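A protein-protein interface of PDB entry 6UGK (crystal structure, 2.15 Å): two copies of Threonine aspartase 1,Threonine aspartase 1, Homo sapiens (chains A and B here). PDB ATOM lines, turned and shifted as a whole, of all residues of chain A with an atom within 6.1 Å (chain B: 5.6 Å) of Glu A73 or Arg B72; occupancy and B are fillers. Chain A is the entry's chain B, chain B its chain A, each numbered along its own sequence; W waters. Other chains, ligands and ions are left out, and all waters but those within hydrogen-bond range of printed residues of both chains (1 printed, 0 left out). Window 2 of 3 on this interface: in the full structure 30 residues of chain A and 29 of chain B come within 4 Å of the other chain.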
ATOM      1  N   GLY A  38     -13.059  -1.786 -23.545  1.00  0.00           N
ATOM      2  CA  GLY A  38     -12.300  -1.176 -24.621  1.00  0.00           C
ATOM      3  C   GLY A  38     -12.075  -2.049 -25.838  1.00  0.00           C
ATOM      4  O   GLY A  38     -11.789  -1.520 -26.918  1.00  0.00           O
ATOM      5  N   ARG A  67      -0.878  -4.876 -29.032  1.00  0.00           N
ATOM      6  CA  ARG A  67      -0.987  -3.466 -28.650  1.00  0.00           C
ATOM      7  C   ARG A  67      -2.287  -2.835 -29.165  1.00  0.00           C
ATOM      8  O   ARG A  67      -2.318  -1.652 -29.522  1.00  0.00           O
ATOM      9  CB  ARG A  67       0.240  -2.675 -29.131  1.00  0.00           C
ATOM     10  N   THR A  68      -3.375  -3.621 -29.189  1.00  0.00           N
ATOM     11  CA  THR A  68      -4.633  -3.193 -29.807  1.00  0.00           C
ATOM     12  C   THR A  68      -5.798  -3.335 -28.838  1.00  0.00           C
ATOM     13  O   THR A  68      -6.079  -4.430 -28.336  1.00  0.00           O
ATOM     14  CB  THR A  68      -4.945  -3.982 -31.084  1.00  0.00           C
ATOM     15  OG1 THR A  68      -3.914  -3.774 -32.055  1.00  0.00           O
ATOM     16  CG2 THR A  68      -6.271  -3.527 -31.672  1.00  0.00           C
ATOM     17  N   ILE A  69      -6.489  -2.233 -28.618  1.00  0.00           N
ATOM     18  CA  ILE A  69      -7.722  -2.175 -27.849  1.00  0.00           C
ATOM     19  C   ILE A  69      -8.760  -1.669 -28.849  1.00  0.00           C
ATOM     20  O   ILE A  69      -8.967  -0.464 -29.025  1.00  0.00           O
ATOM     21  CB  ILE A  69      -7.564  -1.275 -26.618  1.00  0.00           C
ATOM     22  CG1 ILE A  69      -6.522  -1.912 -25.672  1.00  0.00           C
ATOM     23  CG2 ILE A  69      -8.866  -1.032 -25.900  1.00  0.00           C
ATOM     24  CD1 ILE A  69      -6.195  -1.084 -24.461  1.00  0.00           C
ATOM     25  N   LEU A  70      -9.378  -2.608 -29.569  1.00  0.00           N
ATOM     26  CA  LEU A  70      -9.849  -2.308 -30.919  1.00  0.00           C
ATOM     27  C   LEU A  70     -11.058  -1.380 -30.916  1.00  0.00           C
ATOM     28  O   LEU A  70     -11.073  -0.376 -31.633  1.00  0.00           O
ATOM     29  CB  LEU A  70     -10.164  -3.601 -31.675  1.00  0.00           C
ATOM     30  CG  LEU A  70     -10.585  -3.313 -33.116  1.00  0.00           C
ATOM     31  CD1 LEU A  70      -9.425  -2.690 -33.906  1.00  0.00           C
ATOM     32  CD2 LEU A  70     -11.147  -4.549 -33.820  1.00  0.00           C
ATOM     33  N   ALA A  71     -12.102  -1.711 -30.149  1.00  0.00           N
ATOM     34  CA  ALA A  71     -13.319  -0.907 -30.224  1.00  0.00           C
ATOM     35  C   ALA A  71     -13.036   0.538 -29.826  1.00  0.00           C
ATOM     36  O   ALA A  71     -13.455   1.474 -30.507  1.00  0.00           O
ATOM     37  CB  ALA A  71     -14.425  -1.517 -29.357  1.00  0.00           C
ATOM     38  N   ARG A  72     -12.290   0.736 -28.740  1.00  0.00           N
ATOM     39  CA  ARG A  72     -11.921   2.088 -28.324  1.00  0.00           C
ATOM     40  C   ARG A  72     -11.060   2.772 -29.372  1.00  0.00           C
ATOM     41  O   ARG A  72     -11.218   3.973 -29.635  1.00  0.00           O
ATOM     42  CB  ARG A  72     -11.183   2.032 -26.990  1.00  0.00           C
ATOM     43  CG  ARG A  72     -11.007   3.350 -26.278  1.00  0.00           C
ATOM     44  CD  ARG A  72     -10.202   3.076 -25.036  1.00  0.00           C
ATOM     45  NE  ARG A  72     -10.192   4.159 -24.063  1.00  0.00           N
ATOM     46  CZ  ARG A  72      -9.087   4.785 -23.670  1.00  0.00           C
ATOM     47  NH1 ARG A  72      -7.914   4.432 -24.185  1.00  0.00           N
ATOM     48  NH2 ARG A  72      -9.155   5.753 -22.766  1.00  0.00           N
ATOM     49  N   GLU A  73     -10.137   2.031 -29.987  1.00  0.00           N
ATOM     50  CA  GLU A  73      -9.291   2.659 -30.993  1.00  0.00           C
ATOM     51  C   GLU A  73     -10.107   3.098 -32.206  1.00  0.00           C
ATOM     52  O   GLU A  73      -9.847   4.166 -32.775  1.00  0.00           O
ATOM     53  CB  GLU A  73      -8.142   1.726 -31.382  1.00  0.00           C
ATOM     54  CG  GLU A  73      -6.779   2.231 -30.870  1.00  0.00           C
ATOM     55  CD  GLU A  73      -5.769   1.118 -30.597  1.00  0.00           C
ATOM     56  OE1 GLU A  73      -6.138   0.099 -29.971  1.00  0.00           O
ATOM     57  OE2 GLU A  73      -4.597   1.265 -31.007  1.00  0.00           O
ATOM     58  N   CYS A  74     -11.111   2.315 -32.612  1.00  0.00           N
ATOM     59  CA  CYS A  74     -11.964   2.775 -33.712  1.00  0.00           C
ATOM     60  C   CYS A  74     -12.736   4.029 -33.319  1.00  0.00           C
ATOM     61  O   CYS A  74     -12.856   4.966 -34.115  1.00  0.00           O
ATOM     62  CB  CYS A  74     -12.941   1.678 -34.139  1.00  0.00           C
ATOM     63  SG  CYS A  74     -12.160   0.214 -34.852  1.00  0.00           S
ATOM     64  N   SER A  75     -13.292   4.045 -32.104  1.00  0.00           N
ATOM     65  CA  SER A  75     -14.023   5.215 -31.632  1.00  0.00           C
ATOM     66  C   SER A  75     -13.150   6.464 -31.649  1.00  0.00           C
ATOM     67  O   SER A  75     -13.612   7.548 -32.020  1.00  0.00           O
ATOM     68  CB  SER A  75     -14.555   4.957 -30.222  1.00  0.00           C
ATOM     69  OG  SER A  75     -15.157   6.126 -29.693  1.00  0.00           O
ATOM     70  N   HIS A  76     -11.884   6.337 -31.240  1.00  0.00           N
ATOM     71  CA  HIS A  76     -11.003   7.500 -31.273  1.00  0.00           C
ATOM     72  C   HIS A  76     -10.692   7.909 -32.706  1.00  0.00           C
ATOM     73  O   HIS A  76     -10.685   9.101 -33.025  1.00  0.00           O
ATOM     74  CB  HIS A  76      -9.715   7.226 -30.488  1.00  0.00           C
ATOM     75  CG  HIS A  76      -9.909   7.188 -28.997  1.00  0.00           C
ATOM     76  ND1 HIS A  76      -8.867   6.997 -28.113  1.00  0.00           N
ATOM     77  CD2 HIS A  76     -11.024   7.310 -28.238  1.00  0.00           C
ATOM     78  CE1 HIS A  76      -9.331   7.005 -26.875  1.00  0.00           C
ATOM     79  NE2 HIS A  76     -10.638   7.192 -26.923  1.00  0.00           N
ATOM     80  N   ALA A  77     -10.448   6.935 -33.590  1.00  0.00           N
ATOM     81  CA  ALA A  77     -10.147   7.267 -34.981  1.00  0.00           C
ATOM     82  C   ALA A  77     -11.331   7.934 -35.669  1.00  0.00           C
ATOM     83  O   ALA A  77     -11.138   8.752 -36.575  1.00  0.00           O
ATOM     84  CB  ALA A  77      -9.736   6.013 -35.748  1.00  0.00           C
ATOM     85  N   LEU A  78     -12.555   7.601 -35.256  1.00  0.00           N
ATOM     86  CA  LEU A  78     -13.748   8.178 -35.860  1.00  0.00           C
ATOM     87  C   LEU A  78     -14.000   9.612 -35.417  1.00  0.00           C
ATOM     88  O   LEU A  78     -15.019  10.188 -35.813  1.00  0.00           O
ATOM     89  CB  LEU A  78     -14.967   7.301 -35.547  1.00  0.00           C
ATOM     90  CG  LEU A  78     -15.006   5.952 -36.286  1.00  0.00           C
ATOM     91  CD1 LEU A  78     -16.085   5.068 -35.725  1.00  0.00           C
ATOM     92  CD2 LEU A  78     -15.247   6.168 -37.784  1.00  0.00           C
ATOM     93  N   THR A  90      -7.573   2.528 -39.887  1.00  0.00           N
ATOM     94  CA  THR A  90      -7.461   1.770 -38.645  1.00  0.00           C
ATOM     95  C   THR A  90      -7.445   0.275 -38.918  1.00  0.00           C
ATOM     96  O   THR A  90      -6.608  -0.456 -38.375  1.00  0.00           O
ATOM     97  CB  THR A  90      -8.614   2.122 -37.707  1.00  0.00           C
ATOM     98  OG1 THR A  90      -8.673   3.541 -37.537  1.00  0.00           O
ATOM     99  CG2 THR A  90      -8.421   1.452 -36.348  1.00  0.00           C
ATOM    100  N   LYS A  94      -3.979  -2.112 -38.483  1.00  0.00           N
ATOM    101  CA  LYS A  94      -4.113  -3.120 -37.436  1.00  0.00           C
ATOM    102  C   LYS A  94      -4.165  -4.547 -37.966  1.00  0.00           C
ATOM    103  O   LYS A  94      -3.368  -5.388 -37.543  1.00  0.00           O
ATOM    104  CB  LYS A  94      -5.368  -2.842 -36.596  1.00  0.00           C
ATOM    105  CG  LYS A  94      -5.249  -1.644 -35.672  1.00  0.00           C
ATOM    106  CD  LYS A  94      -4.155  -1.869 -34.673  1.00  0.00           C
ATOM    107  CE  LYS A  94      -4.278  -0.920 -33.485  1.00  0.00           C
ATOM    108  NZ  LYS A  94      -3.125  -1.110 -32.551  1.00  0.00           N
ATOM    109  N   GLY B  38      -4.300  -3.573 -20.851  1.00  0.00           N
ATOM    110  CA  GLY B  38      -4.233  -2.124 -20.851  1.00  0.00           C
ATOM    111  C   GLY B  38      -4.468  -1.444 -19.511  1.00  0.00           C
ATOM    112  O   GLY B  38      -4.126  -0.265 -19.365  1.00  0.00           O
ATOM    113  N   CYS B  39      -5.039  -2.135 -18.526  1.00  0.00           N
ATOM    114  CA  CYS B  39      -5.479  -1.479 -17.298  1.00  0.00           C
ATOM    115  C   CYS B  39      -4.506  -1.674 -16.141  1.00  0.00           C
ATOM    116  O   CYS B  39      -4.070  -0.694 -15.529  1.00  0.00           O
ATOM    117  CB  CYS B  39      -6.893  -1.966 -16.917  1.00  0.00           C
ATOM    118  SG  CYS B  39      -8.152  -1.609 -18.233  1.00  0.00           S
ATOM    119  N   CYS B  41      -1.320  -3.211 -16.246  1.00  0.00           N
ATOM    120  CA  CYS B  41       0.082  -3.031 -16.605  1.00  0.00           C
ATOM    121  C   CYS B  41       0.193  -2.865 -18.110  1.00  0.00           C
ATOM    122  O   CYS B  41      -0.750  -3.126 -18.863  1.00  0.00           O
ATOM    123  CB  CYS B  41       0.962  -4.205 -16.137  1.00  0.00           C
ATOM    124  SG  CYS B  41       0.748  -5.795 -17.033  1.00  0.00           S
ATOM    125  N   TRP B  42       1.366  -2.419 -18.542  1.00  0.00           N
ATOM    126  CA  TRP B  42       1.628  -2.227 -19.958  1.00  0.00           C
ATOM    127  C   TRP B  42       3.132  -2.181 -20.134  1.00  0.00           C
ATOM    128  O   TRP B  42       3.838  -1.596 -19.311  1.00  0.00           O
ATOM    129  CB  TRP B  42       1.011  -0.924 -20.485  1.00  0.00           C
ATOM    130  CG  TRP B  42       0.988  -0.842 -21.986  1.00  0.00           C
ATOM    131  CD1 TRP B  42       1.888  -0.212 -22.786  1.00  0.00           C
ATOM    132  CD2 TRP B  42       0.013  -1.426 -22.861  1.00  0.00           C
ATOM    133  NE1 TRP B  42       1.527  -0.345 -24.102  1.00  0.00           N
ATOM    134  CE2 TRP B  42       0.383  -1.090 -24.177  1.00  0.00           C
ATOM    135  CE3 TRP B  42      -1.140  -2.185 -22.654  1.00  0.00           C
ATOM    136  CZ2 TRP B  42      -0.357  -1.488 -25.286  1.00  0.00           C
ATOM    137  CZ3 TRP B  42      -1.875  -2.580 -23.750  1.00  0.00           C
ATOM    138  CH2 TRP B  42      -1.479  -2.226 -25.060  1.00  0.00           C
ATOM    139  N   VAL B  56       4.687   0.060 -17.354  1.00  0.00           N
ATOM    140  CA  VAL B  56       3.778   0.703 -16.405  1.00  0.00           C
ATOM    141  C   VAL B  56       3.057  -0.361 -15.592  1.00  0.00           C
ATOM    142  O   VAL B  56       2.616  -1.366 -16.144  1.00  0.00           O
ATOM    143  CB  VAL B  56       2.729   1.572 -17.131  1.00  0.00           C
ATOM    144  CG1 VAL B  56       1.739   2.171 -16.126  1.00  0.00           C
ATOM    145  CG2 VAL B  56       3.391   2.645 -17.996  1.00  0.00           C
ATOM    146  N   ILE B  69      -8.410   3.075 -18.368  1.00  0.00           N
ATOM    147  CA  ILE B  69      -7.365   2.283 -19.032  1.00  0.00           C
ATOM    148  C   ILE B  69      -5.988   2.874 -18.750  1.00  0.00           C
ATOM    149  O   ILE B  69      -5.229   3.200 -19.674  1.00  0.00           O
ATOM    150  CB  ILE B  69      -7.630   2.180 -20.548  1.00  0.00           C
ATOM    151  CG1 ILE B  69      -9.127   1.931 -20.808  1.00  0.00           C
ATOM    152  CG2 ILE B  69      -6.753   1.090 -21.189  1.00  0.00           C
ATOM    153  CD1 ILE B  69      -9.440   1.196 -22.118  1.00  0.00           C
ATOM    154  N   LEU B  70      -5.655   3.014 -17.462  1.00  0.00           N
ATOM    155  CA  LEU B  70      -4.623   3.965 -17.065  1.00  0.00           C
ATOM    156  C   LEU B  70      -3.228   3.520 -17.484  1.00  0.00           C
ATOM    157  O   LEU B  70      -2.396   4.360 -17.861  1.00  0.00           O
ATOM    158  CB  LEU B  70      -4.667   4.193 -15.557  1.00  0.00           C
ATOM    159  CG  LEU B  70      -3.662   5.256 -15.091  1.00  0.00           C
ATOM    160  CD1 LEU B  70      -3.929   6.621 -15.731  1.00  0.00           C
ATOM    161  CD2 LEU B  70      -3.686   5.380 -13.595  1.00  0.00           C
ATOM    162  N   ALA B  71      -2.931   2.218 -17.381  1.00  0.00           N
ATOM    163  CA  ALA B  71      -1.579   1.755 -17.676  1.00  0.00           C
ATOM    164  C   ALA B  71      -1.187   2.115 -19.103  1.00  0.00           C
ATOM    165  O   ALA B  71      -0.136   2.730 -19.338  1.00  0.00           O
ATOM    166  CB  ALA B  71      -1.462   0.248 -17.444  1.00  0.00           C
ATOM    167  N   ARG B  72      -2.045   1.786 -20.065  1.00  0.00           N
ATOM    168  CA  ARG B  72      -1.759   2.139 -21.450  1.00  0.00           C
ATOM    169  C   ARG B  72      -1.739   3.651 -21.655  1.00  0.00           C
ATOM    170  O   ARG B  72      -0.935   4.170 -22.440  1.00  0.00           O
ATOM    171  CB  ARG B  72      -2.790   1.529 -22.380  1.00  0.00           C
ATOM    172  CG  ARG B  72      -2.355   1.653 -23.813  1.00  0.00           C
ATOM    173  CD  ARG B  72      -3.378   1.137 -24.738  1.00  0.00           C
ATOM    174  NE  ARG B  72      -2.783   0.830 -26.026  1.00  0.00           N
ATOM    175  CZ  ARG B  72      -3.403   0.978 -27.188  1.00  0.00           C
ATOM    176  NH1 ARG B  72      -4.639   1.468 -27.219  1.00  0.00           N
ATOM    177  NH2 ARG B  72      -2.775   0.651 -28.314  1.00  0.00           N
ATOM    178  N   GLU B  73      -2.655   4.365 -21.011  1.00  0.00           N
ATOM    179  CA  GLU B  73      -2.673   5.811 -21.176  1.00  0.00           C
ATOM    180  C   GLU B  73      -1.351   6.411 -20.711  1.00  0.00           C
ATOM    181  O   GLU B  73      -0.783   7.273 -21.381  1.00  0.00           O
ATOM    182  CB  GLU B  73      -3.850   6.405 -20.407  1.00  0.00           C
ATOM    183  CG  GLU B  73      -4.073   7.858 -20.695  1.00  0.00           C
ATOM    184  CD  GLU B  73      -4.677   8.074 -22.069  1.00  0.00           C
ATOM    185  OE1 GLU B  73      -5.495   7.229 -22.491  1.00  0.00           O
ATOM    186  OE2 GLU B  73      -4.322   9.079 -22.723  1.00  0.00           O
ATOM    187  N   CYS B  74      -0.820   5.913 -19.592  1.00  0.00           N
ATOM    188  CA  CYS B  74       0.472   6.384 -19.099  1.00  0.00           C
ATOM    189  C   CYS B  74       1.601   6.065 -20.072  1.00  0.00           C
ATOM    190  O   CYS B  74       2.453   6.918 -20.347  1.00  0.00           O
ATOM    191  CB  CYS B  74       0.755   5.772 -17.734  1.00  0.00           C
ATOM    192  SG  CYS B  74      -0.202   6.505 -16.426  1.00  0.00           S
ATOM    193  N   SER B  75       1.621   4.847 -20.609  1.00  0.00           N
ATOM    194  CA  SER B  75       2.660   4.479 -21.563  1.00  0.00           C
ATOM    195  C   SER B  75       2.634   5.375 -22.804  1.00  0.00           C
ATOM    196  O   SER B  75       3.687   5.772 -23.306  1.00  0.00           O
ATOM    197  CB  SER B  75       2.510   3.011 -21.958  1.00  0.00           C
ATOM    198  OG  SER B  75       3.535   2.660 -22.865  1.00  0.00           O
ATOM    199  N   HIS B  76       1.447   5.700 -23.320  1.00  0.00           N
ATOM    200  CA  HIS B  76       1.388   6.582 -24.488  1.00  0.00           C
ATOM    201  C   HIS B  76       1.838   8.007 -24.142  1.00  0.00           C
ATOM    202  O   HIS B  76       2.572   8.637 -24.907  1.00  0.00           O
ATOM    203  CB  HIS B  76      -0.025   6.598 -25.079  1.00  0.00           C
ATOM    204  CG  HIS B  76      -0.407   5.330 -25.785  1.00  0.00           C
ATOM    205  ND1 HIS B  76       0.411   4.220 -25.826  1.00  0.00           N
ATOM    206  CD2 HIS B  76      -1.522   4.999 -26.480  1.00  0.00           C
ATOM    207  CE1 HIS B  76      -0.183   3.259 -26.511  1.00  0.00           C
ATOM    208  NE2 HIS B  76      -1.355   3.708 -26.922  1.00  0.00           N
ATOM    209  N   ALA B  77       1.434   8.526 -22.984  1.00  0.00           N
ATOM    210  CA  ALA B  77       1.866   9.866 -22.610  1.00  0.00           C
ATOM    211  C   ALA B  77       3.385   9.947 -22.468  1.00  0.00           C
ATOM    212  O   ALA B  77       3.999  10.962 -22.827  1.00  0.00           O
ATOM    213  CB  ALA B  77       1.179  10.284 -21.317  1.00  0.00           C
HETATM  214  O   HOH W   1      -7.042   2.727 -26.389  1.00  0.00           O
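OE1 of Glu B73 is in salt-bridge range of NH2 of Arg A72, at 3.96 Å.
The guanidinium group of Arg B72 lies within hydrogen-bond range of the backbone carbonyl oxygen of Arg A67 (2.6 Å).
The side-chain carboxylate (OE2) of Glu A73 lies within salt-bridge range of the guanidinium group (NH2) of Arg B72 (3.3 Å).
The backbone NH (N) of Ile A69 is in hydrogen-bond range of the side-chain carboxylate (OE1) of Glu A73, at 2.7 Å.
A ring nitrogen (NE2) of His B76 sits at hydrogen-bond distance from the guanidinium group (NE) of Arg B72.
The backbone carbonyl oxygen (O) of Gly A38 sits at hydrogen-bond distance from the backbone NH (N) of Arg A72 (2.9 Å).
The backbone carbonyl oxygen (O) of Gly B38 lies within hydrogen-bond range of the backbone NH (N) of Arg B72 (3.0 Å).
O of Trp B42 is in hydrogen-bond range of N of Val B56 (2.7 Å).
The side-chain carboxylate (OE2) of Glu A73 is in salt-bridge range of the side-chain amino group (NZ) of Lys A94 (3.2 Å).
Among the printed residues, merely in contact across the chains: Arg A72 with Ile B69 (3.6 Å), Ile A69 with Arg B72 (3.6 Å), Arg A67 with Trp B42 (3.8 Å) and Ile A69 with Ile B69 (3.97 Å).
Of the printed residues of chain B, Ile A69 touches Ile B69 and Arg B72.
Glu A73 touches just one residue of chain B: Arg B72 (3.3 Å).
Of the printed residues of chain A, Trp B42 touches Arg A67.
Printed residues of chain A within 4 Å of Ile B69: Ile A69 and Arg A72.
Arg B72 touches three residues of chain A.
Of the printed residues of chain A, Glu B73 touches Arg A72.
Cys B74 touches none of the printed residues of chain A.
The nearest printed residue of chain B that does not touch Glu A73 is His B76 (5.8 Å).
The nearest residue of chain A that does not touch Arg B72 is Thr A68 (4.4 Å).
The nearest printed residue of chain A that does not touch Ile B69 is Gly A38 (4.5 Å).
Hydrophobic or aromatic side chains of chain B within 4 Å of the printed part of chain A: Trp B42 and Ile B69.
Hydrophobic or aromatic side chains of chain A that line the printed part of chain B: Ile A69.
Among the printed residues, 7 pairs touch across the chains.
Among the printed residues, Asp or Glu carboxylates within 4 Å of a Lys or Arg side-chain nitrogen of the other chain: Arg A72 with Glu B73 (3.96 Å) and Glu A73 with Arg B72 (3.3 Å).
Ile A69 touches its own counterpart, Ile B69.
Ile A69 touches Arg B72, and with the chains exchanged Arg A72 touches Ile B69.
Arg A72 touches Glu B73, and with the chains exchanged Glu A73 touches Arg B72.
10 positions are printed for both chains.
Of the 7 pairs that touch across the chains among the printed residues, 5 have their exchanged pair printed and touching as well.
Water W1 bridges the guanidinium group of Arg B72 (2.8 Å) and the guanidinium group of Arg A72 (2.9 Å).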
